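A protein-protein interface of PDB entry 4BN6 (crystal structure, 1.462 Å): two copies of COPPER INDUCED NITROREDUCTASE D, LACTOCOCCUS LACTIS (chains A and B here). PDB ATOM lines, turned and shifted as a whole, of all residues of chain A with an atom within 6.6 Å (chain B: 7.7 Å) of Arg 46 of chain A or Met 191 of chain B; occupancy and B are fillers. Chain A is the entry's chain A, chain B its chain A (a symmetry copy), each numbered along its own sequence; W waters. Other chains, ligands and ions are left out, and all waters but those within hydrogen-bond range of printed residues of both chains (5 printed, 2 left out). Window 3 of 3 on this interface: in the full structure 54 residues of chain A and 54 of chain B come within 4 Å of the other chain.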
ATOM      1  N   VAL A  33     -21.816   2.191   4.130  1.00  0.00           N
ATOM      2  CA  VAL A  33     -22.077   3.593   4.448  1.00  0.00           C
ATOM      3  C   VAL A  33     -20.885   4.464   4.043  1.00  0.00           C
ATOM      4  O   VAL A  33     -21.050   5.516   3.417  1.00  0.00           O
ATOM      5  CB  VAL A  33     -22.365   3.784   5.942  1.00  0.00           C
ATOM      6  CG1 VAL A  33     -22.475   5.260   6.288  1.00  0.00           C
ATOM      7  CG2 VAL A  33     -23.650   3.055   6.330  1.00  0.00           C
ATOM      8  N   ARG A  34     -19.687   4.005   4.380  1.00  0.00           N
ATOM      9  CA  ARG A  34     -18.460   4.745   4.071  1.00  0.00           C
ATOM     10  C   ARG A  34     -18.374   5.124   2.602  1.00  0.00           C
ATOM     11  O   ARG A  34     -18.030   6.257   2.254  1.00  0.00           O
ATOM     12  CB  ARG A  34     -17.247   3.887   4.424  1.00  0.00           C
ATOM     13  CG  ARG A  34     -15.921   4.574   4.268  1.00  0.00           C
ATOM     14  CD  ARG A  34     -14.767   3.618   4.552  1.00  0.00           C
ATOM     15  NE  ARG A  34     -13.492   4.313   4.653  1.00  0.00           N
ATOM     16  CZ  ARG A  34     -13.043   4.918   5.752  1.00  0.00           C
ATOM     17  NH1 ARG A  34     -13.765   4.931   6.866  1.00  0.00           N
ATOM     18  NH2 ARG A  34     -11.882   5.526   5.727  1.00  0.00           N
ATOM     19  N   ASN A  41     -19.959  15.862   0.342  1.00  0.00           N
ATOM     20  CA  ASN A  41     -19.298  14.878   1.197  1.00  0.00           C
ATOM     21  C   ASN A  41     -19.635  15.116   2.663  1.00  0.00           C
ATOM     22  O   ASN A  41     -18.793  14.933   3.545  1.00  0.00           O
ATOM     23  CB  ASN A  41     -17.779  14.910   0.998  1.00  0.00           C
ATOM     24  CG  ASN A  41     -17.094  13.671   1.540  1.00  0.00           C
ATOM     25  OD1 ASN A  41     -17.650  12.579   1.504  1.00  0.00           O
ATOM     26  ND2 ASN A  41     -15.878  13.837   2.048  1.00  0.00           N
ATOM     27  N   SER A  42     -20.882  15.509   2.913  1.00  0.00           N
ATOM     28  CA  SER A  42     -21.340  15.883   4.245  1.00  0.00           C
ATOM     29  C   SER A  42     -21.514  14.699   5.197  1.00  0.00           C
ATOM     30  O   SER A  42     -21.502  14.881   6.416  1.00  0.00           O
ATOM     31  CB  SER A  42     -22.646  16.676   4.142  1.00  0.00           C
ATOM     32  OG  SER A  42     -23.624  15.964   3.397  1.00  0.00           O
ATOM     33  N   GLN A  43     -21.689  13.504   4.647  1.00  0.00           N
ATOM     34  CA  GLN A  43     -21.701  12.281   5.441  1.00  0.00           C
ATOM     35  C   GLN A  43     -22.637  12.421   6.631  1.00  0.00           C
ATOM     36  O   GLN A  43     -22.242  12.221   7.778  1.00  0.00           O
ATOM     37  CB  GLN A  43     -20.285  11.961   5.914  1.00  0.00           C
ATOM     38  CG  GLN A  43     -19.320  11.669   4.776  1.00  0.00           C
ATOM     39  CD  GLN A  43     -17.888  11.659   5.239  1.00  0.00           C
ATOM     40  OE1 GLN A  43     -17.439  10.699   5.862  1.00  0.00           O
ATOM     41  NE2 GLN A  43     -17.169  12.737   4.963  1.00  0.00           N
ATOM     42  N   THR A  44     -23.891  12.756   6.351  1.00  0.00           N
ATOM     43  CA  THR A  44     -24.839  13.056   7.413  1.00  0.00           C
ATOM     44  C   THR A  44     -25.465  11.819   8.068  1.00  0.00           C
ATOM     45  O   THR A  44     -26.115  11.933   9.106  1.00  0.00           O
ATOM     46  CB  THR A  44     -25.958  13.954   6.877  1.00  0.00           C
ATOM     47  OG1 THR A  44     -26.407  13.449   5.609  1.00  0.00           O
ATOM     48  CG2 THR A  44     -25.453  15.371   6.701  1.00  0.00           C
ATOM     49  N   GLY A  45     -25.267  10.645   7.477  1.00  0.00           N
ATOM     50  CA  GLY A  45     -25.833   9.421   8.014  1.00  0.00           C
ATOM     51  C   GLY A  45     -25.197   8.995   9.326  1.00  0.00           C
ATOM     52  O   GLY A  45     -23.979   9.107   9.509  1.00  0.00           O
ATOM     53  N   ARG A  46     -26.035   8.506  10.237  1.00  0.00           N
ATOM     54  CA  ARG A  46     -25.594   7.972  11.524  1.00  0.00           C
ATOM     55  C   ARG A  46     -26.308   6.645  11.750  1.00  0.00           C
ATOM     56  O   ARG A  46     -27.487   6.523  11.433  1.00  0.00           O
ATOM     57  CB  ARG A  46     -25.953   8.923  12.666  1.00  0.00           C
ATOM     58  CG  ARG A  46     -25.440  10.349  12.513  1.00  0.00           C
ATOM     59  CD  ARG A  46     -23.952  10.463  12.761  1.00  0.00           C
ATOM     60  NE  ARG A  46     -23.489  11.841  12.593  1.00  0.00           N
ATOM     61  CZ  ARG A  46     -22.948  12.327  11.476  1.00  0.00           C
ATOM     62  NH1 ARG A  46     -22.770  11.555  10.415  1.00  0.00           N
ATOM     63  NH2 ARG A  46     -22.563  13.593  11.431  1.00  0.00           N
ATOM     64  N   LEU A  47     -25.607   5.661  12.306  1.00  0.00           N
ATOM     65  CA  LEU A  47     -26.189   4.341  12.533  1.00  0.00           C
ATOM     66  C   LEU A  47     -26.090   3.893  13.978  1.00  0.00           C
ATOM     67  O   LEU A  47     -25.062   4.059  14.630  1.00  0.00           O
ATOM     68  CB  LEU A  47     -25.496   3.282  11.680  1.00  0.00           C
ATOM     69  CG  LEU A  47     -25.877   3.136  10.209  1.00  0.00           C
ATOM     70  CD1 LEU A  47     -25.559   4.403   9.430  1.00  0.00           C
ATOM     71  CD2 LEU A  47     -25.161   1.934   9.610  1.00  0.00           C
ATOM     72  N   LEU A  48     -27.184   3.311  14.462  1.00  0.00           N
ATOM     73  CA  LEU A  48     -27.178   2.521  15.679  1.00  0.00           C
ATOM     74  C   LEU A  48     -27.460   1.079  15.281  1.00  0.00           C
ATOM     75  O   LEU A  48     -28.508   0.779  14.705  1.00  0.00           O
ATOM     76  CB  LEU A  48     -28.237   3.032  16.658  1.00  0.00           C
ATOM     77  CG  LEU A  48     -28.439   2.220  17.943  1.00  0.00           C
ATOM     78  CD1 LEU A  48     -27.191   2.265  18.799  1.00  0.00           C
ATOM     79  CD2 LEU A  48     -29.646   2.750  18.708  1.00  0.00           C
ATOM     80  N   LEU A  99     -30.590   1.054  12.866  1.00  0.00           N
ATOM     81  CA  LEU A  99     -31.378   2.272  12.870  1.00  0.00           C
ATOM     82  C   LEU A  99     -30.587   3.377  12.170  1.00  0.00           C
ATOM     83  O   LEU A  99     -29.460   3.698  12.565  1.00  0.00           O
ATOM     84  CB  LEU A  99     -31.767   2.667  14.297  1.00  0.00           C
ATOM     85  CG  LEU A  99     -32.708   1.674  15.001  1.00  0.00           C
ATOM     86  CD1 LEU A  99     -31.915   0.565  15.693  1.00  0.00           C
ATOM     87  CD2 LEU A  99     -33.626   2.373  15.986  1.00  0.00           C
ATOM     88  N   PHE A 100     -31.178   3.916  11.111  1.00  0.00           N
ATOM     89  CA  PHE A 100     -30.562   4.964  10.307  1.00  0.00           C
ATOM     90  C   PHE A 100     -31.092   6.327  10.709  1.00  0.00           C
ATOM     91  O   PHE A 100     -32.301   6.538  10.734  1.00  0.00           O
ATOM     92  CB  PHE A 100     -30.869   4.736   8.828  1.00  0.00           C
ATOM     93  CG  PHE A 100     -30.151   3.563   8.232  1.00  0.00           C
ATOM     94  CD1 PHE A 100     -30.709   2.302   8.270  1.00  0.00           C
ATOM     95  CD2 PHE A 100     -28.918   3.720   7.627  1.00  0.00           C
ATOM     96  CE1 PHE A 100     -30.054   1.221   7.712  1.00  0.00           C
ATOM     97  CE2 PHE A 100     -28.259   2.645   7.068  1.00  0.00           C
ATOM     98  CZ  PHE A 100     -28.826   1.391   7.112  1.00  0.00           C
ATOM     99  N   PHE A 101     -30.178   7.244  11.015  1.00  0.00           N
ATOM    100  CA  PHE A 101     -30.512   8.621  11.356  1.00  0.00           C
ATOM    101  C   PHE A 101     -29.788   9.572  10.409  1.00  0.00           C
ATOM    102  O   PHE A 101     -28.798   9.197   9.771  1.00  0.00           O
ATOM    103  CB  PHE A 101     -30.054   8.988  12.771  1.00  0.00           C
ATOM    104  CG  PHE A 101     -30.481   8.026  13.849  1.00  0.00           C
ATOM    105  CD1 PHE A 101     -29.894   6.773  13.960  1.00  0.00           C
ATOM    106  CD2 PHE A 101     -31.431   8.404  14.787  1.00  0.00           C
ATOM    107  CE1 PHE A 101     -30.269   5.902  14.970  1.00  0.00           C
ATOM    108  CE2 PHE A 101     -31.805   7.536  15.805  1.00  0.00           C
ATOM    109  CZ  PHE A 101     -31.222   6.284  15.887  1.00  0.00           C
ATOM    110  N   GLU A 102     -30.279  10.803  10.340  1.00  0.00           N
ATOM    111  CA  GLU A 102     -29.577  11.890   9.657  1.00  0.00           C
ATOM    112  C   GLU A 102     -29.238  12.973  10.671  1.00  0.00           C
ATOM    113  O   GLU A 102     -30.096  13.401  11.442  1.00  0.00           O
ATOM    114  CB  GLU A 102     -30.432  12.460   8.523  1.00  0.00           C
ATOM    115  CG  GLU A 102     -30.530  11.542   7.317  1.00  0.00           C
ATOM    116  CD  GLU A 102     -29.209  11.429   6.571  1.00  0.00           C
ATOM    117  OE1 GLU A 102     -28.619  12.497   6.267  1.00  0.00           O
ATOM    118  OE2 GLU A 102     -28.774  10.292   6.291  1.00  0.00           O
ATOM    119  N   ASP A 103     -27.981  13.415  10.665  1.00  0.00           N
ATOM    120  CA  ASP A 103     -27.491  14.377  11.650  1.00  0.00           C
ATOM    121  C   ASP A 103     -27.912  15.802  11.287  1.00  0.00           C
ATOM    122  O   ASP A 103     -27.359  16.422  10.380  1.00  0.00           O
ATOM    123  CB  ASP A 103     -25.967  14.291  11.780  1.00  0.00           C
ATOM    124  CG  ASP A 103     -25.439  15.070  12.975  1.00  0.00           C
ATOM    125  OD1 ASP A 103     -26.090  16.056  13.391  1.00  0.00           O
ATOM    126  OD2 ASP A 103     -24.363  14.705  13.498  1.00  0.00           O
ATOM    127  N   VAL A 106     -25.417  18.864  11.252  1.00  0.00           N
ATOM    128  CA  VAL A 106     -24.622  19.042  10.044  1.00  0.00           C
ATOM    129  C   VAL A 106     -25.451  19.706   8.946  1.00  0.00           C
ATOM    130  O   VAL A 106     -24.965  20.588   8.241  1.00  0.00           O
ATOM    131  CB  VAL A 106     -24.050  17.706   9.555  1.00  0.00           C
ATOM    132  CG1 VAL A 106     -23.353  17.877   8.212  1.00  0.00           C
ATOM    133  CG2 VAL A 106     -23.095  17.137  10.589  1.00  0.00           C
ATOM    134  N   ILE A 132     -27.809   5.319   1.786  1.00  0.00           N
ATOM    135  CA  ILE A 132     -27.050   4.444   2.669  1.00  0.00           C
ATOM    136  C   ILE A 132     -27.882   3.251   3.120  1.00  0.00           C
ATOM    137  O   ILE A 132     -27.340   2.167   3.324  1.00  0.00           O
ATOM    138  CB  ILE A 132     -26.402   5.184   3.871  1.00  0.00           C
ATOM    139  CG1 ILE A 132     -27.440   5.777   4.823  1.00  0.00           C
ATOM    140  CG2 ILE A 132     -25.458   6.273   3.364  1.00  0.00           C
ATOM    141  CD1 ILE A 132     -26.823   6.334   6.086  1.00  0.00           C
ATOM    142  N   SER A 169     -29.524  15.639  17.941  1.00  0.00           N
ATOM    143  CA  SER A 169     -29.454  16.008  16.528  1.00  0.00           C
ATOM    144  C   SER A 169     -29.622  14.834  15.562  1.00  0.00           C
ATOM    145  O   SER A 169     -29.772  15.050  14.360  1.00  0.00           O
ATOM    146  CB  SER A 169     -28.128  16.714  16.236  1.00  0.00           C
ATOM    147  OG  SER A 169     -27.049  15.798  16.247  1.00  0.00           O
ATOM    148  N   TRP A 170     -29.591  13.602  16.067  1.00  0.00           N
ATOM    149  CA  TRP A 170     -29.796  12.436  15.209  1.00  0.00           C
ATOM    150  C   TRP A 170     -31.290  12.234  14.942  1.00  0.00           C
ATOM    151  O   TRP A 170     -32.057  11.925  15.859  1.00  0.00           O
ATOM    152  CB  TRP A 170     -29.229  11.164  15.836  1.00  0.00           C
ATOM    153  CG  TRP A 170     -27.722  11.056  15.883  1.00  0.00           C
ATOM    154  CD1 TRP A 170     -26.817  12.075  15.849  1.00  0.00           C
ATOM    155  CD2 TRP A 170     -26.960   9.844  15.990  1.00  0.00           C
ATOM    156  NE1 TRP A 170     -25.536  11.572  15.932  1.00  0.00           N
ATOM    157  CE2 TRP A 170     -25.599  10.207  16.020  1.00  0.00           C
ATOM    158  CE3 TRP A 170     -27.301   8.488  16.066  1.00  0.00           C
ATOM    159  CZ2 TRP A 170     -24.578   9.260  16.117  1.00  0.00           C
ATOM    160  CZ3 TRP A 170     -26.285   7.551  16.160  1.00  0.00           C
ATOM    161  CH2 TRP A 170     -24.940   7.945  16.183  1.00  0.00           C
ATOM    162  N   THR B 189     -12.042  12.645   1.796  1.00  0.00           N
ATOM    163  CA  THR B 189     -11.843  12.216   3.173  1.00  0.00           C
ATOM    164  C   THR B 189     -13.090  11.523   3.723  1.00  0.00           C
ATOM    165  O   THR B 189     -14.170  11.574   3.126  1.00  0.00           O
ATOM    166  CB  THR B 189     -11.505  13.399   4.086  1.00  0.00           C
ATOM    167  OG1 THR B 189     -12.583  14.344   4.069  1.00  0.00           O
ATOM    168  CG2 THR B 189     -10.222  14.080   3.633  1.00  0.00           C
ATOM    169  N   PHE B 190     -12.916  10.872   4.868  1.00  0.00           N
ATOM    170  CA  PHE B 190     -13.989  10.165   5.548  1.00  0.00           C
ATOM    171  C   PHE B 190     -13.999  10.559   7.020  1.00  0.00           C
ATOM    172  O   PHE B 190     -12.946  10.784   7.608  1.00  0.00           O
ATOM    173  CB  PHE B 190     -13.772   8.656   5.438  1.00  0.00           C
ATOM    174  CG  PHE B 190     -13.666   8.155   4.028  1.00  0.00           C
ATOM    175  CD1 PHE B 190     -12.440   8.092   3.394  1.00  0.00           C
ATOM    176  CD2 PHE B 190     -14.788   7.738   3.335  1.00  0.00           C
ATOM    177  CE1 PHE B 190     -12.335   7.634   2.100  1.00  0.00           C
ATOM    178  CE2 PHE B 190     -14.689   7.271   2.029  1.00  0.00           C
ATOM    179  CZ  PHE B 190     -13.460   7.214   1.413  1.00  0.00           C
ATOM    180  N   MET B 191     -15.192  10.666   7.595  1.00  0.00           N
ATOM    181  CA  MET B 191     -15.378  10.841   9.034  1.00  0.00           C
ATOM    182  C   MET B 191     -14.735   9.718   9.830  1.00  0.00           C
ATOM    183  O   MET B 191     -14.530   8.620   9.321  1.00  0.00           O
ATOM    184  CB  MET B 191     -16.860  10.736   9.375  1.00  0.00           C
ATOM    185  CG  MET B 191     -17.727  11.910   9.077  1.00  0.00           C
ATOM    186  SD  MET B 191     -19.364  11.465   9.680  1.00  0.00           S
ATOM    187  CE  MET B 191     -19.091  11.466  11.448  1.00  0.00           C
ATOM    188  N   ASP B 192     -14.491   9.995  11.108  1.00  0.00           N
ATOM    189  CA  ASP B 192     -14.128   8.983  12.097  1.00  0.00           C
ATOM    190  C   ASP B 192     -15.329   8.046  12.297  1.00  0.00           C
ATOM    191  O   ASP B 192     -16.442   8.506  12.559  1.00  0.00           O
ATOM    192  CB  ASP B 192     -13.763   9.700  13.405  1.00  0.00           C
ATOM    193  CG  ASP B 192     -13.203   8.778  14.482  1.00  0.00           C
ATOM    194  OD1 ASP B 192     -13.371   7.543  14.427  1.00  0.00           O
ATOM    195  OD2 ASP B 192     -12.607   9.318  15.434  1.00  0.00           O
ATOM    196  N   ASP B 193     -15.114   6.740  12.140  1.00  0.00           N
ATOM    197  CA  ASP B 193     -16.152   5.740  12.413  1.00  0.00           C
ATOM    198  C   ASP B 193     -16.854   6.005  13.749  1.00  0.00           C
ATOM    199  O   ASP B 193     -18.068   5.841  13.868  1.00  0.00           O
ATOM    200  CB  ASP B 193     -15.551   4.330  12.488  1.00  0.00           C
ATOM    201  CG  ASP B 193     -15.220   3.730  11.130  1.00  0.00           C
ATOM    202  OD1 ASP B 193     -15.594   4.294  10.084  1.00  0.00           O
ATOM    203  OD2 ASP B 193     -14.585   2.649  11.129  1.00  0.00           O
ATOM    204  N   ALA B 194     -16.087   6.391  14.764  1.00  0.00           N
ATOM    205  CA  ALA B 194     -16.629   6.522  16.108  1.00  0.00           C
ATOM    206  C   ALA B 194     -17.691   7.614  16.208  1.00  0.00           C
ATOM    207  O   ALA B 194     -18.495   7.618  17.145  1.00  0.00           O
ATOM    208  CB  ALA B 194     -15.508   6.781  17.104  1.00  0.00           C
ATOM    209  N   ASP B 195     -17.700   8.536  15.253  1.00  0.00           N
ATOM    210  CA  ASP B 195     -18.663   9.637  15.272  1.00  0.00           C
ATOM    211  C   ASP B 195     -19.961   9.333  14.503  1.00  0.00           C
ATOM    212  O   ASP B 195     -20.896  10.135  14.546  1.00  0.00           O
ATOM    213  CB  ASP B 195     -18.029  10.916  14.715  1.00  0.00           C
ATOM    214  CG  ASP B 195     -16.915  11.458  15.602  1.00  0.00           C
ATOM    215  OD1 ASP B 195     -16.975  11.259  16.835  1.00  0.00           O
ATOM    216  OD2 ASP B 195     -15.981  12.080  15.055  1.00  0.00           O
ATOM    217  N   ARG B 196     -20.029   8.200  13.801  1.00  0.00           N
ATOM    218  CA  ARG B 196     -21.246   7.876  13.057  1.00  0.00           C
ATOM    219  C   ARG B 196     -21.755   6.442  13.188  1.00  0.00           C
ATOM    220  O   ARG B 196     -22.843   6.152  12.703  1.00  0.00           O
ATOM    221  CB  ARG B 196     -21.114   8.236  11.572  1.00  0.00           C
ATOM    222  CG  ARG B 196     -20.010   7.515  10.809  1.00  0.00           C
ATOM    223  CD  ARG B 196     -20.195   7.699   9.302  1.00  0.00           C
ATOM    224  NE  ARG B 196     -18.979   7.405   8.549  1.00  0.00           N
ATOM    225  CZ  ARG B 196     -18.819   7.651   7.251  1.00  0.00           C
ATOM    226  NH1 ARG B 196     -19.806   8.167   6.534  1.00  0.00           N
ATOM    227  NH2 ARG B 196     -17.668   7.362   6.664  1.00  0.00           N
ATOM    228  N   PHE B 197     -20.998   5.551  13.829  1.00  0.00           N
ATOM    229  CA  PHE B 197     -21.484   4.190  14.069  1.00  0.00           C
ATOM    230  C   PHE B 197     -21.452   3.854  15.553  1.00  0.00           C
ATOM    231  O   PHE B 197     -20.416   3.980  16.199  1.00  0.00           O
ATOM    232  CB  PHE B 197     -20.651   3.143  13.311  1.00  0.00           C
ATOM    233  CG  PHE B 197     -20.471   3.427  11.843  1.00  0.00           C
ATOM    234  CD1 PHE B 197     -21.532   3.328  10.962  1.00  0.00           C
ATOM    235  CD2 PHE B 197     -19.221   3.740  11.336  1.00  0.00           C
ATOM    236  CE1 PHE B 197     -21.354   3.577   9.611  1.00  0.00           C
ATOM    237  CE2 PHE B 197     -19.044   3.984   9.996  1.00  0.00           C
ATOM    238  CZ  PHE B 197     -20.104   3.895   9.129  1.00  0.00           C
ATOM    239  N   ILE B 198     -22.596   3.446  16.092  1.00  0.00           N
ATOM    240  CA  ILE B 198     -22.670   2.880  17.431  1.00  0.00           C
ATOM    241  C   ILE B 198     -23.182   1.450  17.328  1.00  0.00           C
ATOM    242  O   ILE B 198     -24.205   1.183  16.695  1.00  0.00           O
ATOM    243  CB  ILE B 198     -23.619   3.673  18.346  1.00  0.00           C
ATOM    244  CG1 ILE B 198     -23.158   5.125  18.451  1.00  0.00           C
ATOM    245  CG2 ILE B 198     -23.696   3.018  19.731  1.00  0.00           C
ATOM    246  CD1 ILE B 198     -24.136   6.031  19.166  1.00  0.00           C
HETATM  247  O   HOH W   1     -14.555  13.872   6.013  1.00  0.00           O
HETATM  248  O   HOH W   2     -16.013   3.037   7.731  1.00  0.00           O
HETATM  249  O   HOH W   3     -18.225   8.322   4.034  1.00  0.00           O
HETATM  250  O   HOH W   4     -13.071  15.404   1.054  1.00  0.00           O
HETATM  251  O   HOH W   5     -22.449   8.664   7.246  1.00  0.00           O
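The guanidinium group (NH1) of Arg 46 of chain A sits at hydrogen-bond distance from the side-chain sulfur (SD) of Met 191 of chain B.
OE1 of Gln 43 of chain A lies within hydrogen-bond range of N of Met 191 of chain B, at 2.8 Å.
The backbone carbonyl oxygen (O) of Leu 47 of chain A is in hydrogen-bond range of the backbone NH (N) of Ile 198 of chain B (2.9 Å).
OD1 of Asp 193 of chain B is in salt-bridge range of NH1 of Arg 34 of chain A.
The side-chain amide oxygen of Gln 43 of chain A is in hydrogen-bond range of the guanidinium group of Arg 196 of chain B (3.4 Å).
The backbone NH of Leu 47 of chain A lies within hydrogen-bond range of the backbone carbonyl oxygen of Arg 196 of chain B, 2.8 Å away.
The side-chain amide nitrogen (ND2) of Asn 41 of chain A lies within hydrogen-bond range of the backbone carbonyl oxygen (O) of Thr 189 of chain B (3.0 Å).
O of Gln 43 of chain A lies within hydrogen-bond range of NH1 of Arg 46 of chain A, at 2.8 Å.
The backbone NH (N) of Phe 101 of chain A is in hydrogen-bond range of the backbone carbonyl oxygen (O) of Arg 46 of chain A.
The backbone carbonyl oxygen (O) of Asn 41 of chain A sits at hydrogen-bond distance from the side-chain amide nitrogen (NE2) of Gln 43 of chain A, 3.1 Å away.
NH2 of Arg 46 of chain A is in salt-bridge range of OD2 of Asp 103 of chain A (3.0 Å).
The backbone carbonyl oxygen (O) of Leu 48 of chain A sits at hydrogen-bond distance from the backbone NH (N) of Leu 99 of chain A, at 2.8 Å.
No position is printed for both chains.
Of the 19 pairs that touch across the chains among the printed residues, none has its exchanged pair printed and touching as well.
Of the 10 printed residues of chain B, 8 touch a printed residue of chain A.
Printed residues of chain A that touch a printed residue of chain B: Val 33, Arg 34, Asn 41, Gln 43, Gly 45, Arg 46, Leu 47, Leu 48 and Trp 170.
Printed residues of chain B within 4 Å of Gln 43 of chain A: Thr 189, Phe 190, Met 191 and Arg 196.
Gly 45 of chain A touches just one residue of chain B: Arg 196.
Arg 46 of chain A touches three residues of chain B.
Val 106 of chain A touches none of the printed residues of chain B.
Of the printed residues of chain B, Trp 170 of chain A touches Ile 198.
Met 191 of chain B touches just these residues of chain A: Gln 43 (2.8 Å) and Arg 46 (3.5 Å).
Ala 194 of chain B touches none of the printed residues of chain A.
The nearest residue of chain B that does not touch Arg 46 of chain A is Phe 197 of chain B (5.7 Å).
The nearest residue of chain A that does not touch Met 191 of chain B is Arg 34 of chain A (4.5 Å).
The nearest printed residue of chain A that does not touch Ile 198 of chain B is Arg 46 of chain A (6.5 Å).
Among the printed residues, merely in contact across the chains: Val 33 of chain A with Arg 196 of chain B (3.95 Å), Val 33 of chain A with Phe 197 of chain B (3.8 Å), Arg 34 of chain A with Phe 190 of chain B (3.5 Å), Arg 34 of chain A with Arg 196 of chain B (3.8 Å), Gln 43 of chain A with Thr 189 of chain B (3.7 Å), Gln 43 of chain A with Phe 190 of chain B (3.5 Å), Gly 45 of chain A with Arg 196 of chain B (3.6 Å), Arg 46 of chain A with Asp 195 of chain B (3.6 Å), Arg 46 of chain A with Arg 196 of chain B (3.5 Å), Leu 47 of chain A with Phe 197 of chain B (3.6 Å), Leu 48 of chain A with Ile 198 of chain B (3.4 Å) and Trp 170 of chain A with Ile 198 of chain B (3.6 Å).
Water W2 bridges the side-chain carboxylate of Asp 193 of chain B (2.7 Å) and the guanidinium group of Arg 34 of chain A (3.1 Å).
Water W3 lies within hydrogen-bond range of the backbone carbonyl oxygen (O) of Arg 34 of chain A, the guanidinium group (NH2) of Arg 196 of chain B and the side-chain amide oxygen (OE1) of Gln 43 of chain A.
Water W5 bridges O of Gly 45 of chain A and NH1 of Arg 196 of chain B.
Water W1 bridges the side-chain hydroxyl (OG1) of Thr 189 of chain B and the side-chain amide nitrogen (NE2) of Gln 43 of chain A.
Water W4 lies within hydrogen-bond range of N of Thr 189 of chain B (3.0 Å) and ND2 of Asn 41 of chain A (3.4 Å).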
